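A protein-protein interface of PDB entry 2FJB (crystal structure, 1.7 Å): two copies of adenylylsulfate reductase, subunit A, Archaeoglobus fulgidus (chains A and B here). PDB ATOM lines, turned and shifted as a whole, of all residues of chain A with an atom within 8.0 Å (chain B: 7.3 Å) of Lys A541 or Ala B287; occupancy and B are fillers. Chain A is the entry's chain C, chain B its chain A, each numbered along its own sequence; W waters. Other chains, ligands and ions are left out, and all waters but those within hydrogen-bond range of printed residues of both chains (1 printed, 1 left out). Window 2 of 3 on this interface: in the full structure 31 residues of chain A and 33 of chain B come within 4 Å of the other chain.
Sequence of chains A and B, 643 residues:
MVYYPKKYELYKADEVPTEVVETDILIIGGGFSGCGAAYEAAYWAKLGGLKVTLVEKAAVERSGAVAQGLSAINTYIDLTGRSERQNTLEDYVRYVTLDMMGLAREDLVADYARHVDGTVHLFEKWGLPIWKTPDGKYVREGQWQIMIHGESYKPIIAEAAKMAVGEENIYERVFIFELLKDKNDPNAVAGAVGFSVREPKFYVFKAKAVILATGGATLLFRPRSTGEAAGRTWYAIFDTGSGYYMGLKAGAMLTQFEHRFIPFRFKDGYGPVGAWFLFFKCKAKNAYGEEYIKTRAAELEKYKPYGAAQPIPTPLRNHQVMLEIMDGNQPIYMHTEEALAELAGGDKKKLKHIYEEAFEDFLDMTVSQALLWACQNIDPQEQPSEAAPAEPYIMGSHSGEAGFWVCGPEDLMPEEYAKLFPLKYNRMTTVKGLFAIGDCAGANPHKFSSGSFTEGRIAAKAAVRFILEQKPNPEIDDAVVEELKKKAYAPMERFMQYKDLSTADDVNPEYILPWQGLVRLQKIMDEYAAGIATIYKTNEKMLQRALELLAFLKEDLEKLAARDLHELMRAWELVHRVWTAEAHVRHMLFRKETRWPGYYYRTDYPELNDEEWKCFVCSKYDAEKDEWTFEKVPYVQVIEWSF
Of the 15 printed residues of chain B, 5 touch a printed residue of chain A.
Hydrophobic or aromatic side chains of chain B that line the printed part of chain A: Ala B287, Tyr B288 and Pro B331.
Along chain B the printed residues that touch a printed residue of chain A span positions 287 to 331.
Of the 15 printed residues of chain A, 4 touch a printed residue of chain B.
Printed residues of chain A that touch a printed residue of chain B: Asn A539, Lys A541, Met A542 and Asp A604.
Among the printed residues, 7 pairs touch across the chains.
Water W1 lies within hydrogen-bond range of the side-chain hydroxyl of Tyr B288, the backbone NH of Lys A541, the side-chain amide oxygen of Asn A539 and the backbone NH of Glu A540.
The side-chain amide oxygen of Asn B286 lies within hydrogen-bond range of the backbone NH of Tyr B288, at 2.9 Å.
The side-chain amide oxygen (OD1) of Asn A539 sits at hydrogen-bond distance from the backbone NH (N) of Met A542, at 2.8 Å.
NH2 of Arg A602 lies within salt-bridge range of OD2 of Asp A604, 2.8 Å away.
N of Lys A541 sits at hydrogen-bond distance from OD1 of Asn A539, at 2.9 Å.
N of Ala B287 lies within hydrogen-bond range of O of Asn B329, at 2.9 Å.
The side-chain amino group (NZ) of Lys A541 lies close to the side-chain amide oxygen (OE1) of Gln A544.
Lys A541 touches two residues of chain B.
Ala B287 touches just one residue of chain A: Lys A541.
Of the printed residues of chain B, Asp A604 touches Tyr B288.
Of the printed residues of chain B, Met A542 touches Gln B330.
Printed residues of chain A within 4 Å of Gln B330: Asn A539 and Met A542.
Printed residues of chain B within 4 Å of Asn A539: Tyr B288, Gly B328 and Gln B330.
Of the printed residues of chain A, Pro B331 touches Lys A541 (3.8 Å).
Gly B289 touches none of the printed residues of chain A.
Arg A602 touches none of the printed residues of chain B.
The nearest residue of chain B that does not touch Lys A541 is Gln B330 (4.4 Å).
No position is printed for both chains.
Of the 7 pairs that touch across the chains among the printed residues, none has its exchanged pair printed and touching as well.
O of Gln B330 is in hydrogen-bond range of ND2 of Asn A539, 3.0 Å away.
ND2 of Asn A539 is in hydrogen-bond range of O of Gly B328 (2.9 Å).
Among the printed residues, merely in contact across the chains: Asn A539 with Tyr B288 (3.8 Å), Lys A541 with Ala B287 (3.6 Å), Lys A541 with Pro B331 (3.8 Å), Met A542 with Gln B330 (3.3 Å) and Asp A604 with Tyr B288 (3.7 Å).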
ATOM      1  N   TYR A 528       6.096  24.336  17.113  1.00  0.00           N
ATOM      2  CA  TYR A 528       6.375  23.053  17.747  1.00  0.00           C
ATOM      3  C   TYR A 528       5.780  22.813  19.129  1.00  0.00           C
ATOM      4  O   TYR A 528       5.658  21.664  19.559  1.00  0.00           O
ATOM      5  CB  TYR A 528       7.891  22.836  17.841  1.00  0.00           C
ATOM      6  CG  TYR A 528       8.589  22.834  16.504  1.00  0.00           C
ATOM      7  CD1 TYR A 528       9.089  24.015  15.954  1.00  0.00           C
ATOM      8  CD2 TYR A 528       8.727  21.655  15.774  1.00  0.00           C
ATOM      9  CE1 TYR A 528       9.711  24.021  14.705  1.00  0.00           C
ATOM     10  CE2 TYR A 528       9.342  21.650  14.526  1.00  0.00           C
ATOM     11  CZ  TYR A 528       9.831  22.835  13.999  1.00  0.00           C
ATOM     12  OH  TYR A 528      10.436  22.832  12.763  1.00  0.00           O
ATOM     13  N   THR A 538       0.477  19.070  19.488  1.00  0.00           N
ATOM     14  CA  THR A 538       1.903  18.783  19.488  1.00  0.00           C
ATOM     15  C   THR A 538       2.104  17.307  19.819  1.00  0.00           C
ATOM     16  O   THR A 538       1.140  16.591  20.103  1.00  0.00           O
ATOM     17  CB  THR A 538       2.682  19.664  20.504  1.00  0.00           C
ATOM     18  OG1 THR A 538       4.089  19.495  20.292  1.00  0.00           O
ATOM     19  CG2 THR A 538       2.346  19.281  21.935  1.00  0.00           C
ATOM     20  N   ASN A 539       3.350  16.850  19.742  1.00  0.00           N
ATOM     21  CA  ASN A 539       3.685  15.463  20.060  1.00  0.00           C
ATOM     22  C   ASN A 539       5.139  15.411  20.517  1.00  0.00           C
ATOM     23  O   ASN A 539       5.815  16.443  20.552  1.00  0.00           O
ATOM     24  CB  ASN A 539       3.462  14.541  18.843  1.00  0.00           C
ATOM     25  CG  ASN A 539       4.296  14.937  17.634  1.00  0.00           C
ATOM     26  OD1 ASN A 539       5.477  15.253  17.757  1.00  0.00           O
ATOM     27  ND2 ASN A 539       3.681  14.905  16.449  1.00  0.00           N
ATOM     28  N   GLU A 540       5.618  14.222  20.871  1.00  0.00           N
ATOM     29  CA  GLU A 540       6.991  14.062  21.337  1.00  0.00           C
ATOM     30  C   GLU A 540       8.042  14.580  20.359  1.00  0.00           C
ATOM     31  O   GLU A 540       8.972  15.282  20.761  1.00  0.00           O
ATOM     32  CB  GLU A 540       7.283  12.589  21.646  1.00  0.00           C
ATOM     33  CG  GLU A 540       8.710  12.333  22.116  1.00  0.00           C
ATOM     34  CD  GLU A 540       9.012  10.859  22.292  1.00  0.00           C
ATOM     35  OE1 GLU A 540       8.916  10.107  21.299  1.00  0.00           O
ATOM     36  OE2 GLU A 540       9.344  10.454  23.425  1.00  0.00           O
ATOM     37  N   LYS A 541       7.898  14.234  19.082  1.00  0.00           N
ATOM     38  CA  LYS A 541       8.853  14.651  18.062  1.00  0.00           C
ATOM     39  C   LYS A 541       8.916  16.166  17.921  1.00  0.00           C
ATOM     40  O   LYS A 541      10.007  16.747  17.861  1.00  0.00           O
ATOM     41  CB  LYS A 541       8.488  14.020  16.713  1.00  0.00           C
ATOM     42  CG  LYS A 541       8.417  12.493  16.717  1.00  0.00           C
ATOM     43  CD  LYS A 541       9.794  11.843  16.614  1.00  0.00           C
ATOM     44  CE  LYS A 541      10.655  12.109  17.837  1.00  0.00           C
ATOM     45  NZ  LYS A 541      12.029  11.541  17.692  1.00  0.00           N
ATOM     46  N   MET A 542       7.755  16.805  17.875  1.00  0.00           N
ATOM     47  CA  MET A 542       7.711  18.254  17.749  1.00  0.00           C
ATOM     48  C   MET A 542       8.330  18.919  18.976  1.00  0.00           C
ATOM     49  O   MET A 542       9.111  19.863  18.859  1.00  0.00           O
ATOM     50  CB  MET A 542       6.258  18.707  17.604  1.00  0.00           C
ATOM     51  CG  MET A 542       5.503  17.983  16.504  1.00  0.00           C
ATOM     52  SD  MET A 542       3.837  18.617  16.213  1.00  0.00           S
ATOM     53  CE  MET A 542       4.057  20.388  16.541  1.00  0.00           C
ATOM     54  N   LEU A 543       7.984  18.419  20.156  1.00  0.00           N
ATOM     55  CA  LEU A 543       8.523  18.980  21.387  1.00  0.00           C
ATOM     56  C   LEU A 543      10.034  18.799  21.459  1.00  0.00           C
ATOM     57  O   LEU A 543      10.746  19.691  21.916  1.00  0.00           O
ATOM     58  CB  LEU A 543       7.849  18.332  22.598  1.00  0.00           C
ATOM     59  CG  LEU A 543       6.359  18.674  22.718  1.00  0.00           C
ATOM     60  CD1 LEU A 543       5.720  17.810  23.797  1.00  0.00           C
ATOM     61  CD2 LEU A 543       6.192  20.160  23.040  1.00  0.00           C
ATOM     62  N   GLN A 544      10.528  17.652  21.001  1.00  0.00           N
ATOM     63  CA  GLN A 544      11.964  17.413  21.016  1.00  0.00           C
ATOM     64  C   GLN A 544      12.659  18.376  20.059  1.00  0.00           C
ATOM     65  O   GLN A 544      13.735  18.887  20.365  1.00  0.00           O
ATOM     66  CB  GLN A 544      12.279  15.962  20.642  1.00  0.00           C
ATOM     67  CG  GLN A 544      11.810  14.966  21.691  1.00  0.00           C
ATOM     68  CD  GLN A 544      12.187  13.535  21.366  1.00  0.00           C
ATOM     69  OE1 GLN A 544      11.977  13.064  20.250  1.00  0.00           O
ATOM     70  NE2 GLN A 544      12.736  12.831  22.349  1.00  0.00           N
ATOM     71  N   ARG A 545      12.046  18.631  18.905  1.00  0.00           N
ATOM     72  CA  ARG A 545      12.633  19.562  17.949  1.00  0.00           C
ATOM     73  C   ARG A 545      12.611  20.968  18.554  1.00  0.00           C
ATOM     74  O   ARG A 545      13.532  21.756  18.347  1.00  0.00           O
ATOM     75  CB  ARG A 545      11.862  19.539  16.623  1.00  0.00           C
ATOM     76  CG  ARG A 545      12.443  20.458  15.545  1.00  0.00           C
ATOM     77  CD  ARG A 545      13.959  20.272  15.389  1.00  0.00           C
ATOM     78  NE  ARG A 545      14.492  21.029  14.257  1.00  0.00           N
ATOM     79  CZ  ARG A 545      15.787  21.217  14.022  1.00  0.00           C
ATOM     80  NH1 ARG A 545      16.695  20.704  14.843  1.00  0.00           N
ATOM     81  NH2 ARG A 545      16.176  21.910  12.959  1.00  0.00           N
ATOM     82  N   ALA A 546      11.559  21.281  19.305  1.00  0.00           N
ATOM     83  CA  ALA A 546      11.475  22.589  19.947  1.00  0.00           C
ATOM     84  C   ALA A 546      12.676  22.764  20.878  1.00  0.00           C
ATOM     85  O   ALA A 546      13.285  23.827  20.914  1.00  0.00           O
ATOM     86  CB  ALA A 546      10.169  22.719  20.737  1.00  0.00           C
ATOM     87  N   LEU A 547      13.026  21.720  21.627  1.00  0.00           N
ATOM     88  CA  LEU A 547      14.166  21.811  22.535  1.00  0.00           C
ATOM     89  C   LEU A 547      15.465  22.033  21.763  1.00  0.00           C
ATOM     90  O   LEU A 547      16.335  22.786  22.203  1.00  0.00           O
ATOM     91  CB  LEU A 547      14.277  20.550  23.402  1.00  0.00           C
ATOM     92  CG  LEU A 547      13.150  20.340  24.418  1.00  0.00           C
ATOM     93  CD1 LEU A 547      13.384  19.030  25.166  1.00  0.00           C
ATOM     94  CD2 LEU A 547      13.103  21.515  25.404  1.00  0.00           C
ATOM     95  N   GLU A 548      15.599  21.388  20.610  1.00  0.00           N
ATOM     96  CA  GLU A 548      16.799  21.561  19.801  1.00  0.00           C
ATOM     97  C   GLU A 548      16.915  23.001  19.308  1.00  0.00           C
ATOM     98  O   GLU A 548      17.995  23.597  19.352  1.00  0.00           O
ATOM     99  CB  GLU A 548      16.780  20.597  18.609  1.00  0.00           C
ATOM    100  CG  GLU A 548      16.983  19.146  19.012  1.00  0.00           C
ATOM    101  CD  GLU A 548      16.772  18.175  17.864  1.00  0.00           C
ATOM    102  OE1 GLU A 548      16.639  18.625  16.707  1.00  0.00           O
ATOM    103  OE2 GLU A 548      16.744  16.954  18.124  1.00  0.00           O
ATOM    104  N   LEU A 589       6.442  17.755  27.451  1.00  0.00           N
ATOM    105  CA  LEU A 589       7.062  16.521  26.979  1.00  0.00           C
ATOM    106  C   LEU A 589       6.971  15.424  28.043  1.00  0.00           C
ATOM    107  O   LEU A 589       6.737  14.252  27.730  1.00  0.00           O
ATOM    108  CB  LEU A 589       8.530  16.782  26.621  1.00  0.00           C
ATOM    109  CG  LEU A 589       9.385  15.609  26.129  1.00  0.00           C
ATOM    110  CD1 LEU A 589       8.735  14.946  24.919  1.00  0.00           C
ATOM    111  CD2 LEU A 589      10.773  16.131  25.769  1.00  0.00           C
ATOM    112  N   ARG A 602      -1.843  16.455  22.960  1.00  0.00           N
ATOM    113  CA  ARG A 602      -0.673  15.669  22.599  1.00  0.00           C
ATOM    114  C   ARG A 602      -1.297  14.592  21.722  1.00  0.00           C
ATOM    115  O   ARG A 602      -1.996  13.705  22.208  1.00  0.00           O
ATOM    116  CB  ARG A 602       0.016  15.055  23.820  1.00  0.00           C
ATOM    117  CG  ARG A 602       0.995  16.018  24.470  1.00  0.00           C
ATOM    118  CD  ARG A 602       2.058  15.315  25.282  1.00  0.00           C
ATOM    119  NE  ARG A 602       2.888  14.409  24.485  1.00  0.00           N
ATOM    120  CZ  ARG A 602       4.008  13.852  24.937  1.00  0.00           C
ATOM    121  NH1 ARG A 602       4.426  14.123  26.167  1.00  0.00           N
ATOM    122  NH2 ARG A 602       4.700  13.010  24.177  1.00  0.00           N
ATOM    123  N   ASP A 604      -0.016  12.184  20.354  1.00  0.00           N
ATOM    124  CA  ASP A 604       0.536  10.855  20.607  1.00  0.00           C
ATOM    125  C   ASP A 604       0.010  10.241  21.912  1.00  0.00           C
ATOM    126  O   ASP A 604       0.169   9.046  22.152  1.00  0.00           O
ATOM    127  CB  ASP A 604       2.078  10.884  20.569  1.00  0.00           C
ATOM    128  CG  ASP A 604       2.691  11.946  21.466  1.00  0.00           C
ATOM    129  OD1 ASP A 604       1.991  12.899  21.866  1.00  0.00           O
ATOM    130  OD2 ASP A 604       3.904  11.833  21.748  1.00  0.00           O
ATOM    131  N   LYS B 285       8.651  11.205   4.785  1.00  0.00           N
ATOM    132  CA  LYS B 285       7.989  10.401   5.811  1.00  0.00           C
ATOM    133  C   LYS B 285       7.548  11.292   6.962  1.00  0.00           C
ATOM    134  O   LYS B 285       8.145  12.343   7.193  1.00  0.00           O
ATOM    135  CB  LYS B 285       8.945   9.330   6.342  1.00  0.00           C
ATOM    136  CG  LYS B 285       9.497   8.403   5.273  1.00  0.00           C
ATOM    137  CD  LYS B 285      10.497   7.419   5.869  1.00  0.00           C
ATOM    138  CE  LYS B 285      11.038   6.474   4.810  1.00  0.00           C
ATOM    139  NZ  LYS B 285      11.979   5.476   5.401  1.00  0.00           N
ATOM    140  N   ASN B 286       6.503  10.887   7.677  1.00  0.00           N
ATOM    141  CA  ASN B 286       6.045  11.692   8.800  1.00  0.00           C
ATOM    142  C   ASN B 286       6.942  11.451  10.004  1.00  0.00           C
ATOM    143  O   ASN B 286       7.935  10.721   9.918  1.00  0.00           O
ATOM    144  CB  ASN B 286       4.574  11.405   9.146  1.00  0.00           C
ATOM    145  CG  ASN B 286       4.328   9.970   9.558  1.00  0.00           C
ATOM    146  OD1 ASN B 286       5.237   9.271  10.004  1.00  0.00           O
ATOM    147  ND2 ASN B 286       3.078   9.528   9.429  1.00  0.00           N
ATOM    148  N   ALA B 287       6.593  12.066  11.127  1.00  0.00           N
ATOM    149  CA  ALA B 287       7.392  11.960  12.341  1.00  0.00           C
ATOM    150  C   ALA B 287       7.629  10.535  12.825  1.00  0.00           C
ATOM    151  O   ALA B 287       8.587  10.276  13.554  1.00  0.00           O
ATOM    152  CB  ALA B 287       6.741  12.778  13.450  1.00  0.00           C
ATOM    153  N   TYR B 288       6.765   9.614  12.413  1.00  0.00           N
ATOM    154  CA  TYR B 288       6.886   8.227  12.846  1.00  0.00           C
ATOM    155  C   TYR B 288       7.535   7.305  11.826  1.00  0.00           C
ATOM    156  O   TYR B 288       7.571   6.087  12.014  1.00  0.00           O
ATOM    157  CB  TYR B 288       5.509   7.699  13.243  1.00  0.00           C
ATOM    158  CG  TYR B 288       4.847   8.585  14.268  1.00  0.00           C
ATOM    159  CD1 TYR B 288       3.849   9.489  13.900  1.00  0.00           C
ATOM    160  CD2 TYR B 288       5.271   8.575  15.598  1.00  0.00           C
ATOM    161  CE1 TYR B 288       3.293  10.365  14.831  1.00  0.00           C
ATOM    162  CE2 TYR B 288       4.724   9.446  16.536  1.00  0.00           C
ATOM    163  CZ  TYR B 288       3.737  10.339  16.145  1.00  0.00           C
ATOM    164  OH  TYR B 288       3.210  11.219  17.065  1.00  0.00           O
ATOM    165  N   GLY B 289       8.045   7.890  10.748  1.00  0.00           N
ATOM    166  CA  GLY B 289       8.714   7.099   9.731  1.00  0.00           C
ATOM    167  C   GLY B 289       7.821   6.498   8.665  1.00  0.00           C
ATOM    168  O   GLY B 289       8.268   5.641   7.903  1.00  0.00           O
ATOM    169  N   GLU B 290       6.568   6.934   8.601  1.00  0.00           N
ATOM    170  CA  GLU B 290       5.644   6.410   7.600  1.00  0.00           C
ATOM    171  C   GLU B 290       5.710   7.203   6.305  1.00  0.00           C
ATOM    172  O   GLU B 290       5.680   8.434   6.326  1.00  0.00           O
ATOM    173  CB  GLU B 290       4.202   6.465   8.106  1.00  0.00           C
ATOM    174  CG  GLU B 290       3.929   5.652   9.346  1.00  0.00           C
ATOM    175  CD  GLU B 290       2.466   5.687   9.725  1.00  0.00           C
ATOM    176  OE1 GLU B 290       1.944   6.791   9.987  1.00  0.00           O
ATOM    177  OE2 GLU B 290       1.837   4.609   9.757  1.00  0.00           O
ATOM    178  N   TYR B 292       3.831   8.555   3.882  1.00  0.00           N
ATOM    179  CA  TYR B 292       2.418   8.836   3.697  1.00  0.00           C
ATOM    180  C   TYR B 292       1.842   8.778   2.288  1.00  0.00           C
ATOM    181  O   TYR B 292       0.623   8.734   2.138  1.00  0.00           O
ATOM    182  CB  TYR B 292       2.067  10.163   4.372  1.00  0.00           C
ATOM    183  CG  TYR B 292       2.896  11.321   3.903  1.00  0.00           C
ATOM    184  CD1 TYR B 292       2.520  12.061   2.789  1.00  0.00           C
ATOM    185  CD2 TYR B 292       4.073  11.667   4.567  1.00  0.00           C
ATOM    186  CE1 TYR B 292       3.290  13.116   2.347  1.00  0.00           C
ATOM    187  CE2 TYR B 292       4.854  12.719   4.132  1.00  0.00           C
ATOM    188  CZ  TYR B 292       4.458  13.440   3.027  1.00  0.00           C
ATOM    189  OH  TYR B 292       5.225  14.493   2.609  1.00  0.00           O
ATOM    190  N   GLU B 324      -1.892  14.416   7.058  1.00  0.00           N
ATOM    191  CA  GLU B 324      -0.861  14.115   8.046  1.00  0.00           C
ATOM    192  C   GLU B 324      -0.736  15.263   9.039  1.00  0.00           C
ATOM    193  O   GLU B 324      -0.565  15.043  10.238  1.00  0.00           O
ATOM    194  CB  GLU B 324       0.489  13.893   7.360  1.00  0.00           C
ATOM    195  CG  GLU B 324       0.602  12.566   6.620  1.00  0.00           C
ATOM    196  CD  GLU B 324       0.484  11.376   7.550  1.00  0.00           C
ATOM    197  OE1 GLU B 324       1.211  11.343   8.565  1.00  0.00           O
ATOM    198  OE2 GLU B 324      -0.334  10.476   7.268  1.00  0.00           O
ATOM    199  N   GLY B 328      -1.718  15.516  13.159  1.00  0.00           N
ATOM    200  CA  GLY B 328      -0.626  15.848  14.059  1.00  0.00           C
ATOM    201  C   GLY B 328       0.586  14.943  13.917  1.00  0.00           C
ATOM    202  O   GLY B 328       1.236  14.611  14.908  1.00  0.00           O
ATOM    203  N   ASN B 329       0.909  14.555  12.686  1.00  0.00           N
ATOM    204  CA  ASN B 329       2.049  13.674  12.462  1.00  0.00           C
ATOM    205  C   ASN B 329       3.322  14.381  12.007  1.00  0.00           C
ATOM    206  O   ASN B 329       4.198  13.765  11.396  1.00  0.00           O
ATOM    207  CB  ASN B 329       1.678  12.564  11.473  1.00  0.00           C
ATOM    208  CG  ASN B 329       0.578  11.659  12.006  1.00  0.00           C
ATOM    209  OD1 ASN B 329       0.372  11.568  13.216  1.00  0.00           O
ATOM    210  ND2 ASN B 329      -0.124  10.981  11.104  1.00  0.00           N
ATOM    211  N   GLN B 330       3.424  15.675  12.294  1.00  0.00           N
ATOM    212  CA  GLN B 330       4.625  16.425  11.945  1.00  0.00           C
ATOM    213  C   GLN B 330       5.666  16.147  13.029  1.00  0.00           C
ATOM    214  O   GLN B 330       5.324  15.715  14.129  1.00  0.00           O
ATOM    215  CB  GLN B 330       4.323  17.925  11.861  1.00  0.00           C
ATOM    216  CG  GLN B 330       3.540  18.303  10.613  1.00  0.00           C
ATOM    217  CD  GLN B 330       3.309  19.798  10.481  1.00  0.00           C
ATOM    218  OE1 GLN B 330       2.526  20.389  11.226  1.00  0.00           O
ATOM    219  NE2 GLN B 330       3.998  20.418   9.531  1.00  0.00           N
ATOM    220  N   PRO B 331       6.951  16.400  12.739  1.00  0.00           N
ATOM    221  CA  PRO B 331       7.453  16.928  11.469  1.00  0.00           C
ATOM    222  C   PRO B 331       7.419  15.938  10.315  1.00  0.00           C
ATOM    223  O   PRO B 331       7.472  14.723  10.509  1.00  0.00           O
ATOM    224  CB  PRO B 331       8.901  17.319  11.790  1.00  0.00           C
ATOM    225  CG  PRO B 331       8.957  17.362  13.303  1.00  0.00           C
ATOM    226  CD  PRO B 331       8.053  16.239  13.699  1.00  0.00           C
ATOM    227  N   ILE B 332       7.326  16.482   9.109  1.00  0.00           N
ATOM    228  CA  ILE B 332       7.368  15.674   7.899  1.00  0.00           C
ATOM    229  C   ILE B 332       8.817  15.840   7.442  1.00  0.00           C
ATOM    230  O   ILE B 332       9.326  16.965   7.377  1.00  0.00           O
ATOM    231  CB  ILE B 332       6.412  16.219   6.819  1.00  0.00           C
ATOM    232  CG1 ILE B 332       4.961  16.040   7.276  1.00  0.00           C
ATOM    233  CG2 ILE B 332       6.677  15.525   5.488  1.00  0.00           C
ATOM    234  CD1 ILE B 332       4.594  14.621   7.668  1.00  0.00           C
ATOM    235  N   TYR B 333       9.484  14.726   7.144  1.00  0.00           N
ATOM    236  CA  TYR B 333      10.886  14.757   6.737  1.00  0.00           C
ATOM    237  C   TYR B 333      11.217  14.296   5.331  1.00  0.00           C
ATOM    238  O   TYR B 333      10.630  13.345   4.816  1.00  0.00           O
ATOM    239  CB  TYR B 333      11.742  13.896   7.673  1.00  0.00           C
ATOM    240  CG  TYR B 333      11.881  14.416   9.074  1.00  0.00           C
ATOM    241  CD1 TYR B 333      11.059  13.949  10.099  1.00  0.00           C
ATOM    242  CD2 TYR B 333      12.837  15.382   9.380  1.00  0.00           C
ATOM    243  CE1 TYR B 333      11.190  14.434  11.396  1.00  0.00           C
ATOM    244  CE2 TYR B 333      12.975  15.870  10.666  1.00  0.00           C
ATOM    245  CZ  TYR B 333      12.152  15.395  11.669  1.00  0.00           C
ATOM    246  OH  TYR B 333      12.292  15.893  12.942  1.00  0.00           O
ATOM    247  N   HIS B 335      13.953  12.529   3.659  1.00  0.00           N
ATOM    248  CA  HIS B 335      15.102  11.734   4.083  1.00  0.00           C
ATOM    249  C   HIS B 335      16.256  11.703   3.090  1.00  0.00           C
ATOM    250  O   HIS B 335      16.544  10.686   2.451  1.00  0.00           O
ATOM    251  CB  HIS B 335      14.644  10.324   4.451  1.00  0.00           C
ATOM    252  CG  HIS B 335      13.977  10.256   5.789  1.00  0.00           C
ATOM    253  ND1 HIS B 335      14.688  10.221   6.969  1.00  0.00           N
ATOM    254  CD2 HIS B 335      12.670  10.305   6.137  1.00  0.00           C
ATOM    255  CE1 HIS B 335      13.848  10.253   7.988  1.00  0.00           C
ATOM    256  NE2 HIS B 335      12.617  10.306   7.511  1.00  0.00           N
HETATM  257  O   HOH W   1       5.783  12.058  18.285  1.00  0.00           O
